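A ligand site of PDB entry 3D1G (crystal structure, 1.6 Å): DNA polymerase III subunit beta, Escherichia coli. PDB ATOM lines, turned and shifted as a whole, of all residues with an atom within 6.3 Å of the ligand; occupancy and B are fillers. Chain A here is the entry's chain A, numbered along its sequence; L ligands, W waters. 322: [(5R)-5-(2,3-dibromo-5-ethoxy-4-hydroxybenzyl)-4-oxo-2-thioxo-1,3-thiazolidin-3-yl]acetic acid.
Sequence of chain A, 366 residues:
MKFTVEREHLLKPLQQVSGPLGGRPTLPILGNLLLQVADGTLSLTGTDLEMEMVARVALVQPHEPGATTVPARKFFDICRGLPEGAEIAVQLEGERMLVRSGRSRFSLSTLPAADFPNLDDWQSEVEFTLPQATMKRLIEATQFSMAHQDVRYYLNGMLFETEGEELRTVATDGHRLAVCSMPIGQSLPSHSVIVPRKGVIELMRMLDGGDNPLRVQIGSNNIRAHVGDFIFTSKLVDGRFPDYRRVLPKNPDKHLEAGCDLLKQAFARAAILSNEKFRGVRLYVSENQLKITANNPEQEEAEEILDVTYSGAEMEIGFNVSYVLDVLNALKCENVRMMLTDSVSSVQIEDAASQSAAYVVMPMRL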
ATOM      1  N   ARG A 152     -19.185  38.465   1.834  1.00  0.00           N
ATOM      2  CA  ARG A 152     -17.955  37.697   2.011  1.00  0.00           C
ATOM      3  C   ARG A 152     -17.839  36.987   0.669  1.00  0.00           C
ATOM      4  O   ARG A 152     -18.170  35.815   0.529  1.00  0.00           O
ATOM      5  CB  ARG A 152     -18.113  36.681   3.154  1.00  0.00           C
ATOM      6  CG  ARG A 152     -18.360  37.325   4.504  1.00  0.00           C
ATOM      7  CD  ARG A 152     -18.575  36.279   5.606  1.00  0.00           C
ATOM      8  NE  ARG A 152     -17.364  35.541   5.935  1.00  0.00           N
ATOM      9  CZ  ARG A 152     -17.312  34.554   6.822  1.00  0.00           C
ATOM     10  NH1 ARG A 152     -18.422  34.182   7.445  1.00  0.00           N
ATOM     11  NH2 ARG A 152     -16.167  33.926   7.088  1.00  0.00           N
ATOM     12  N   TYR A 154     -15.558  35.641  -1.035  1.00  0.00           N
ATOM     13  CA  TYR A 154     -14.782  34.421  -1.154  1.00  0.00           C
ATOM     14  C   TYR A 154     -15.605  33.172  -0.836  1.00  0.00           C
ATOM     15  O   TYR A 154     -15.102  32.055  -0.962  1.00  0.00           O
ATOM     16  CB  TYR A 154     -13.553  34.489  -0.248  1.00  0.00           C
ATOM     17  CG  TYR A 154     -13.849  35.031   1.140  1.00  0.00           C
ATOM     18  CD1 TYR A 154     -14.424  34.227   2.121  1.00  0.00           C
ATOM     19  CD2 TYR A 154     -13.546  36.357   1.472  1.00  0.00           C
ATOM     20  CE1 TYR A 154     -14.698  34.718   3.395  1.00  0.00           C
ATOM     21  CE2 TYR A 154     -13.815  36.862   2.736  1.00  0.00           C
ATOM     22  CZ  TYR A 154     -14.378  36.034   3.698  1.00  0.00           C
ATOM     23  OH  TYR A 154     -14.644  36.520   4.957  1.00  0.00           O
ATOM     24  N   LEU A 155     -16.850  33.367  -0.428  1.00  0.00           N
ATOM     25  CA  LEU A 155     -17.739  32.237  -0.128  1.00  0.00           C
ATOM     26  C   LEU A 155     -18.674  31.922  -1.300  1.00  0.00           C
ATOM     27  O   LEU A 155     -19.440  30.970  -1.241  1.00  0.00           O
ATOM     28  CB  LEU A 155     -18.601  32.546   1.099  1.00  0.00           C
ATOM     29  CG  LEU A 155     -17.908  32.743   2.444  1.00  0.00           C
ATOM     30  CD1 LEU A 155     -18.973  32.896   3.535  1.00  0.00           C
ATOM     31  CD2 LEU A 155     -17.010  31.559   2.754  1.00  0.00           C
ATOM     32  N   THR A 172     -19.223  26.838   2.104  1.00  0.00           N
ATOM     33  CA  THR A 172     -19.913  27.363   3.254  1.00  0.00           C
ATOM     34  C   THR A 172     -20.458  28.756   2.978  1.00  0.00           C
ATOM     35  O   THR A 172     -19.960  29.467   2.100  1.00  0.00           O
ATOM     36  CB  THR A 172     -19.004  27.434   4.502  1.00  0.00           C
ATOM     37  OG1 THR A 172     -19.784  27.824   5.633  1.00  0.00           O
ATOM     38  CG2 THR A 172     -17.893  28.471   4.304  1.00  0.00           C
ATOM     39  N   ASP A 173     -21.495  29.123   3.707  1.00  0.00           N
ATOM     40  CA  ASP A 173     -22.080  30.452   3.570  1.00  0.00           C
ATOM     41  C   ASP A 173     -21.972  31.158   4.912  1.00  0.00           C
ATOM     42  O   ASP A 173     -22.586  32.197   5.144  1.00  0.00           O
ATOM     43  CB  ASP A 173     -23.530  30.372   3.089  1.00  0.00           C
ATOM     44  CG  ASP A 173     -24.413  29.533   4.004  1.00  0.00           C
ATOM     45  OD1 ASP A 173     -25.547  29.231   3.577  1.00  0.00           O
ATOM     46  OD2 ASP A 173     -23.994  29.197   5.127  1.00  0.00           O
ATOM     47  N   GLY A 174     -21.172  30.569   5.804  1.00  0.00           N
ATOM     48  CA  GLY A 174     -20.974  31.140   7.121  1.00  0.00           C
ATOM     49  C   GLY A 174     -21.908  30.616   8.202  1.00  0.00           C
ATOM     50  O   GLY A 174     -21.675  30.851   9.386  1.00  0.00           O
ATOM     51  N   HIS A 175     -22.964  29.916   7.786  1.00  0.00           N
ATOM     52  CA  HIS A 175     -23.945  29.370   8.718  1.00  0.00           C
ATOM     53  C   HIS A 175     -23.975  27.842   8.695  1.00  0.00           C
ATOM     54  O   HIS A 175     -24.332  27.218   9.694  1.00  0.00           O
ATOM     55  CB  HIS A 175     -25.329  29.925   8.377  1.00  0.00           C
ATOM     56  CG  HIS A 175     -25.399  31.417   8.393  1.00  0.00           C
ATOM     57  ND1 HIS A 175     -25.225  32.154   9.537  1.00  0.00           N
ATOM     58  CD2 HIS A 175     -25.568  32.310   7.387  1.00  0.00           C
ATOM     59  CE1 HIS A 175     -25.301  33.443   9.246  1.00  0.00           C
ATOM     60  NE2 HIS A 175     -25.503  33.559   7.942  1.00  0.00           N
ATOM     61  N   ARG A 176     -23.632  27.266   7.553  1.00  0.00           N
ATOM     62  CA  ARG A 176     -23.560  25.814   7.426  1.00  0.00           C
ATOM     63  C   ARG A 176     -22.408  25.513   6.480  1.00  0.00           C
ATOM     64  O   ARG A 176     -22.092  26.317   5.606  1.00  0.00           O
ATOM     65  CB  ARG A 176     -24.888  25.215   6.927  1.00  0.00           C
ATOM     66  CG  ARG A 176     -25.619  25.967   5.810  1.00  0.00           C
ATOM     67  CD  ARG A 176     -25.076  25.687   4.425  1.00  0.00           C
ATOM     68  NE  ARG A 176     -25.890  26.368   3.407  1.00  0.00           N
ATOM     69  CZ  ARG A 176     -27.035  25.903   2.917  1.00  0.00           C
ATOM     70  NH1 ARG A 176     -27.532  24.737   3.327  1.00  0.00           N
ATOM     71  NH2 ARG A 176     -27.706  26.619   2.020  1.00  0.00           N
ATOM     72  N   LEU A 177     -21.778  24.359   6.659  1.00  0.00           N
ATOM     73  CA  LEU A 177     -20.632  24.012   5.844  1.00  0.00           C
ATOM     74  C   LEU A 177     -20.634  22.554   5.408  1.00  0.00           C
ATOM     75  O   LEU A 177     -21.166  21.685   6.104  1.00  0.00           O
ATOM     76  CB  LEU A 177     -19.354  24.335   6.646  1.00  0.00           C
ATOM     77  CG  LEU A 177     -17.983  23.970   6.087  1.00  0.00           C
ATOM     78  CD1 LEU A 177     -16.944  24.954   6.609  1.00  0.00           C
ATOM     79  CD2 LEU A 177     -17.617  22.553   6.503  1.00  0.00           C
ATOM     80  N   PHE A 241     -10.208  31.421   1.861  1.00  0.00           N
ATOM     81  CA  PHE A 241     -11.341  30.690   2.398  1.00  0.00           C
ATOM     82  C   PHE A 241     -11.259  30.487   3.917  1.00  0.00           C
ATOM     83  O   PHE A 241     -10.176  30.460   4.487  1.00  0.00           O
ATOM     84  CB  PHE A 241     -11.392  29.312   1.705  1.00  0.00           C
ATOM     85  CG  PHE A 241     -12.735  28.654   1.746  1.00  0.00           C
ATOM     86  CD1 PHE A 241     -13.738  29.046   0.870  1.00  0.00           C
ATOM     87  CD2 PHE A 241     -13.007  27.634   2.669  1.00  0.00           C
ATOM     88  CE1 PHE A 241     -14.991  28.447   0.905  1.00  0.00           C
ATOM     89  CE2 PHE A 241     -14.266  27.031   2.715  1.00  0.00           C
ATOM     90  CZ  PHE A 241     -15.254  27.439   1.827  1.00  0.00           C
ATOM     91  N   PRO A 242     -12.417  30.357   4.584  1.00  0.00           N
ATOM     92  CA  PRO A 242     -12.401  30.162   6.030  1.00  0.00           C
ATOM     93  C   PRO A 242     -11.712  28.863   6.482  1.00  0.00           C
ATOM     94  O   PRO A 242     -11.540  27.921   5.707  1.00  0.00           O
ATOM     95  CB  PRO A 242     -13.895  30.215   6.417  1.00  0.00           C
ATOM     96  CG  PRO A 242     -14.607  29.922   5.144  1.00  0.00           C
ATOM     97  CD  PRO A 242     -13.790  30.625   4.106  1.00  0.00           C
ATOM     98  N   ASP A 243     -11.309  28.843   7.750  1.00  0.00           N
ATOM     99  CA  ASP A 243     -10.628  27.704   8.387  1.00  0.00           C
ATOM    100  C   ASP A 243     -11.663  26.618   8.701  1.00  0.00           C
ATOM    101  O   ASP A 243     -12.162  26.537   9.815  1.00  0.00           O
ATOM    102  CB  ASP A 243      -9.965  28.224   9.679  1.00  0.00           C
ATOM    103  CG  ASP A 243      -9.149  27.166  10.417  1.00  0.00           C
ATOM    104  OD1 ASP A 243      -9.120  25.992   9.996  1.00  0.00           O
ATOM    105  OD2 ASP A 243      -8.535  27.529  11.436  1.00  0.00           O
ATOM    106  N   TYR A 244     -11.973  25.786   7.711  1.00  0.00           N
ATOM    107  CA  TYR A 244     -12.984  24.751   7.888  1.00  0.00           C
ATOM    108  C   TYR A 244     -12.614  23.711   8.948  1.00  0.00           C
ATOM    109  O   TYR A 244     -13.492  23.127   9.570  1.00  0.00           O
ATOM    110  CB  TYR A 244     -13.308  24.068   6.557  1.00  0.00           C
ATOM    111  CG  TYR A 244     -12.226  23.175   6.029  1.00  0.00           C
ATOM    112  CD1 TYR A 244     -12.148  21.836   6.438  1.00  0.00           C
ATOM    113  CD2 TYR A 244     -11.268  23.653   5.144  1.00  0.00           C
ATOM    114  CE1 TYR A 244     -11.134  21.006   5.987  1.00  0.00           C
ATOM    115  CE2 TYR A 244     -10.247  22.826   4.681  1.00  0.00           C
ATOM    116  CZ  TYR A 244     -10.190  21.509   5.112  1.00  0.00           C
ATOM    117  OH  TYR A 244      -9.185  20.676   4.664  1.00  0.00           O
ATOM    118  N   ARG A 246     -11.356  24.225  11.823  1.00  0.00           N
ATOM    119  CA  ARG A 246     -11.781  24.714  13.125  1.00  0.00           C
ATOM    120  C   ARG A 246     -13.295  24.600  13.259  1.00  0.00           C
ATOM    121  O   ARG A 246     -13.830  24.482  14.366  1.00  0.00           O
ATOM    122  CB  ARG A 246     -11.378  26.177  13.322  1.00  0.00           C
ATOM    123  CG  ARG A 246     -11.707  26.722  14.712  1.00  0.00           C
ATOM    124  CD  ARG A 246     -11.345  28.194  14.806  1.00  0.00           C
ATOM    125  NE  ARG A 246     -11.553  28.752  16.147  1.00  0.00           N
ATOM    126  CZ  ARG A 246     -12.720  29.210  16.605  1.00  0.00           C
ATOM    127  NH1 ARG A 246     -13.805  29.184  15.832  1.00  0.00           N
ATOM    128  NH2 ARG A 246     -12.798  29.691  17.844  1.00  0.00           N
ATOM    129  N   VAL A 247     -13.991  24.627  12.132  1.00  0.00           N
ATOM    130  CA  VAL A 247     -15.443  24.530  12.120  1.00  0.00           C
ATOM    131  C   VAL A 247     -15.929  23.155  12.579  1.00  0.00           C
ATOM    132  O   VAL A 247     -16.951  23.055  13.261  1.00  0.00           O
ATOM    133  CB  VAL A 247     -16.005  24.838  10.727  1.00  0.00           C
ATOM    134  CG1 VAL A 247     -17.488  24.490  10.653  1.00  0.00           C
ATOM    135  CG2 VAL A 247     -15.799  26.314  10.424  1.00  0.00           C
ATOM    136  N   SER A 345     -23.968  24.746  20.398  1.00  0.00           N
ATOM    137  CA  SER A 345     -22.890  24.309  19.524  1.00  0.00           C
ATOM    138  C   SER A 345     -23.444  23.725  18.225  1.00  0.00           C
ATOM    139  O   SER A 345     -24.598  23.281  18.173  1.00  0.00           O
ATOM    140  CB  SER A 345     -22.031  23.257  20.227  1.00  0.00           C
ATOM    141  OG  SER A 345     -21.433  23.776  21.401  1.00  0.00           O
ATOM    142  N   SER A 346     -22.622  23.716  17.190  1.00  0.00           N
ATOM    143  CA  SER A 346     -23.067  23.188  15.910  1.00  0.00           C
ATOM    144  C   SER A 346     -23.183  21.675  15.973  1.00  0.00           C
ATOM    145  O   SER A 346     -22.708  21.038  16.920  1.00  0.00           O
ATOM    146  CB  SER A 346     -22.080  23.568  14.814  1.00  0.00           C
ATOM    147  OG  SER A 346     -22.071  24.962  14.613  1.00  0.00           O
ATOM    148  N   VAL A 347     -23.822  21.109  14.953  1.00  0.00           N
ATOM    149  CA  VAL A 347     -23.982  19.666  14.840  1.00  0.00           C
ATOM    150  C   VAL A 347     -23.208  19.219  13.603  1.00  0.00           C
ATOM    151  O   VAL A 347     -23.139  19.939  12.611  1.00  0.00           O
ATOM    152  CB  VAL A 347     -25.471  19.277  14.674  1.00  0.00           C
ATOM    153  CG1 VAL A 347     -26.034  19.883  13.385  1.00  0.00           C
ATOM    154  CG2 VAL A 347     -25.614  17.765  14.638  1.00  0.00           C
ATOM    155  N   VAL A 360     -21.597  20.562   8.689  1.00  0.00           N
ATOM    156  CA  VAL A 360     -21.693  21.225   9.982  1.00  0.00           C
ATOM    157  C   VAL A 360     -22.728  22.341   9.886  1.00  0.00           C
ATOM    158  O   VAL A 360     -22.663  23.183   8.986  1.00  0.00           O
ATOM    159  CB  VAL A 360     -20.347  21.820  10.431  1.00  0.00           C
ATOM    160  CG1 VAL A 360     -20.472  22.384  11.842  1.00  0.00           C
ATOM    161  CG2 VAL A 360     -19.257  20.759  10.391  1.00  0.00           C
ATOM    162  N   VAL A 361     -23.672  22.345  10.821  1.00  0.00           N
ATOM    163  CA  VAL A 361     -24.708  23.362  10.824  1.00  0.00           C
ATOM    164  C   VAL A 361     -24.787  24.081  12.155  1.00  0.00           C
ATOM    165  O   VAL A 361     -24.849  23.442  13.204  1.00  0.00           O
ATOM    166  CB  VAL A 361     -26.084  22.746  10.520  1.00  0.00           C
ATOM    167  CG1 VAL A 361     -27.138  23.858  10.387  1.00  0.00           C
ATOM    168  CG2 VAL A 361     -26.019  21.944   9.219  1.00  0.00           C
ATOM    169  N   MET A 362     -24.767  25.403  12.118  1.00  0.00           N
ATOM    170  CA  MET A 362     -24.870  26.213  13.325  1.00  0.00           C
ATOM    171  C   MET A 362     -26.249  26.041  13.928  1.00  0.00           C
ATOM    172  O   MET A 362     -27.231  25.830  13.212  1.00  0.00           O
ATOM    173  CB  MET A 362     -24.658  27.693  13.010  1.00  0.00           C
ATOM    174  CG  MET A 362     -23.226  28.121  12.742  1.00  0.00           C
ATOM    175  SD  MET A 362     -23.179  29.914  12.566  1.00  0.00           S
ATOM    176  CE  MET A 362     -21.430  30.196  12.464  1.00  0.00           C
ATOM    177  N   PRO A 363     -26.348  26.139  15.257  1.00  0.00           N
ATOM    178  CA  PRO A 363     -27.644  25.999  15.915  1.00  0.00           C
ATOM    179  C   PRO A 363     -28.360  27.347  15.900  1.00  0.00           C
ATOM    180  O   PRO A 363     -27.742  28.376  15.649  1.00  0.00           O
ATOM    181  CB  PRO A 363     -27.262  25.572  17.321  1.00  0.00           C
ATOM    182  CG  PRO A 363     -26.028  26.390  17.563  1.00  0.00           C
ATOM    183  CD  PRO A 363     -25.263  26.211  16.255  1.00  0.00           C
HETATM  184  C10 322 L   1     -12.541  31.992   9.207  1.00  0.00           C
HETATM  185  C8  322 L   1     -14.357  31.822  12.014  1.00  0.00           C
HETATM  186  C9  322 L   1     -13.490  32.927   9.904  1.00  0.00           C
HETATM  187  C4  322 L   1     -17.892  28.683  12.585  1.00  0.00           C
HETATM  188  C5  322 L   1     -18.003  28.806  11.156  1.00  0.00           C
HETATM  189  C6  322 L   1     -17.112  29.777  10.383  1.00  0.00           C
HETATM  190  C3  322 L   1     -18.692  27.737  13.322  1.00  0.00           C
HETATM  191  C2  322 L   1     -17.821  28.311  15.554  1.00  0.00           C
HETATM  192  C1  322 L   1     -18.036  27.861  16.981  1.00  0.00           C
HETATM  193  C7  322 L   1     -16.608  31.052  11.003  1.00  0.00           C
HETATM  194 BR1  322 L   1     -19.168  28.125   8.581  1.00  0.00          BR
HETATM  195 BR2  322 L   1     -20.925  25.874  10.290  1.00  0.00          BR
HETATM  196  N1  322 L   1     -14.509  32.175  10.677  1.00  0.00           N
HETATM  197  S1  322 L   1     -15.734  30.930  12.566  1.00  0.00           S
HETATM  198  O1  322 L   1     -18.688  27.532  14.716  1.00  0.00           O
HETATM  199  C11 322 L   1     -15.696  31.778  10.056  1.00  0.00           C
HETATM  200  C12 322 L   1     -18.949  27.972  10.483  1.00  0.00           C
HETATM  201  C13 322 L   1     -19.713  27.027  11.197  1.00  0.00           C
HETATM  202  C14 322 L   1     -19.590  26.913  12.603  1.00  0.00           C
HETATM  203  O2  322 L   1     -12.411  30.786   9.422  1.00  0.00           O
HETATM  204  S2  322 L   1     -13.082  32.158  13.045  1.00  0.00           S
HETATM  205  O3  322 L   1     -11.814  32.672   8.279  1.00  0.00           O
HETATM  206  O4  322 L   1     -16.019  31.984   8.895  1.00  0.00           O
HETATM  207  O5  322 L   1     -20.343  25.986  13.296  1.00  0.00           O
HETATM  208  O   HOH W   1     -13.144  34.317   6.640  1.00  0.00           O
HETATM  209  O   HOH W   2      -9.399  31.444   8.218  1.00  0.00           O
HETATM  210  O   HOH W   3     -14.372  27.877  13.478  1.00  0.00           O
HETATM  211  O   HOH W   4     -16.150  30.860  16.991  1.00  0.00           O
HETATM  212  O   HOH W   5     -17.713  30.828   6.913  1.00  0.00           O
HETATM  213  O   HOH W   6     -14.291  32.952  15.924  1.00  0.00           O
HETATM  214  O   HOH W   7     -21.383  26.999  16.131  1.00  0.00           O
HETATM  215  O   HOH W   8     -12.911  28.821  11.332  1.00  0.00           O
HETATM  216  O   HOH W   9     -15.948  25.838  15.257  1.00  0.00           O
HETATM  217  O   HOH W  10     -18.448  24.486  14.831  1.00  0.00           O
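The side-chain hydroxyl (OG) of Ser 346 sits at hydrogen-bond distance from an oxygen (O5) of the ligand (2.4 Å).
NH2 of Arg 152 sits at hydrogen-bond distance from O4 of the ligand, at 2.7 Å.
N of Asp 243 sits at hydrogen-bond distance from O2 of the ligand (2.8 Å).
The side-chain hydroxyl (OG) of Ser 346 sits close to the backbone carbonyl oxygen (O) of Val 361.
NE of Arg 152 sits at hydrogen-bond distance from OH of Tyr 154 (3.1 Å).
The side-chain carboxylate (OD1) of Asp 243 sits at hydrogen-bond distance from the backbone NH (N) of Arg 246.
OG1 of Thr 172 sits at hydrogen-bond distance from N of Gly 174, at 3.1 Å.
OG1 of Thr 172 sits at hydrogen-bond distance from O of Arg 176 (2.8 Å).
The backbone carbonyl oxygen of Val 360 lies within hydrogen-bond range of the backbone NH of Leu 177 (2.8 Å).
The backbone NH of Met 362 sits at hydrogen-bond distance from the backbone carbonyl oxygen of His 175 (3.1 Å).
The backbone NH of His 175 sits at hydrogen-bond distance from the side-chain carboxylate of Asp 173 (2.9 Å).
Thr 172 touches the ligand.
Gly 174 touches the ligand (C to BR1, 3.7 Å).
O of His 175 touches BR2 of the ligand, at 3.7 Å.
CA of Arg 176 touches BR2 of the ligand, 3.9 Å away.
CB of Pro 242 touches O2 of the ligand, 3.4 Å away.
Val 247 touches the ligand (CG2 to C5, 3.4 Å).
Val 360 touches the ligand (O to BR2, 3.5 Å).
CG of Met 362 touches O5 of the ligand, at 3.6 Å.
Of the 22 residues printed, 11 come within 4 Å of the ligand.
The nearest printed residue that does not touch the ligand is Leu 177 (4.03 Å).
Water W1 lies within hydrogen-bond range of an oxygen (O3) of the ligand, the guanidinium group (NH2) of Arg 152 and the side-chain hydroxyl (OH) of Tyr 154.
Water W2 lies within hydrogen-bond range of O3 of the ligand (2.7 Å) and N of Asp 243 (3.3 Å).
Water W8 bridges O2 of the ligand and O of Asp 243.
Water W7 lies within hydrogen-bond range of the side-chain hydroxyl (OG) of Ser 346 (2.6 Å) and an oxygen (O1) of the ligand (3.1 Å).
Water W9 bridges the backbone carbonyl oxygen (O) of Arg 246 (2.7 Å) and an oxygen (O1) of the ligand (3.3 Å).
Water W3 lies within hydrogen-bond range of NH1 of Arg 246 (2.8 Å) and S1 of the ligand (3.5 Å).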
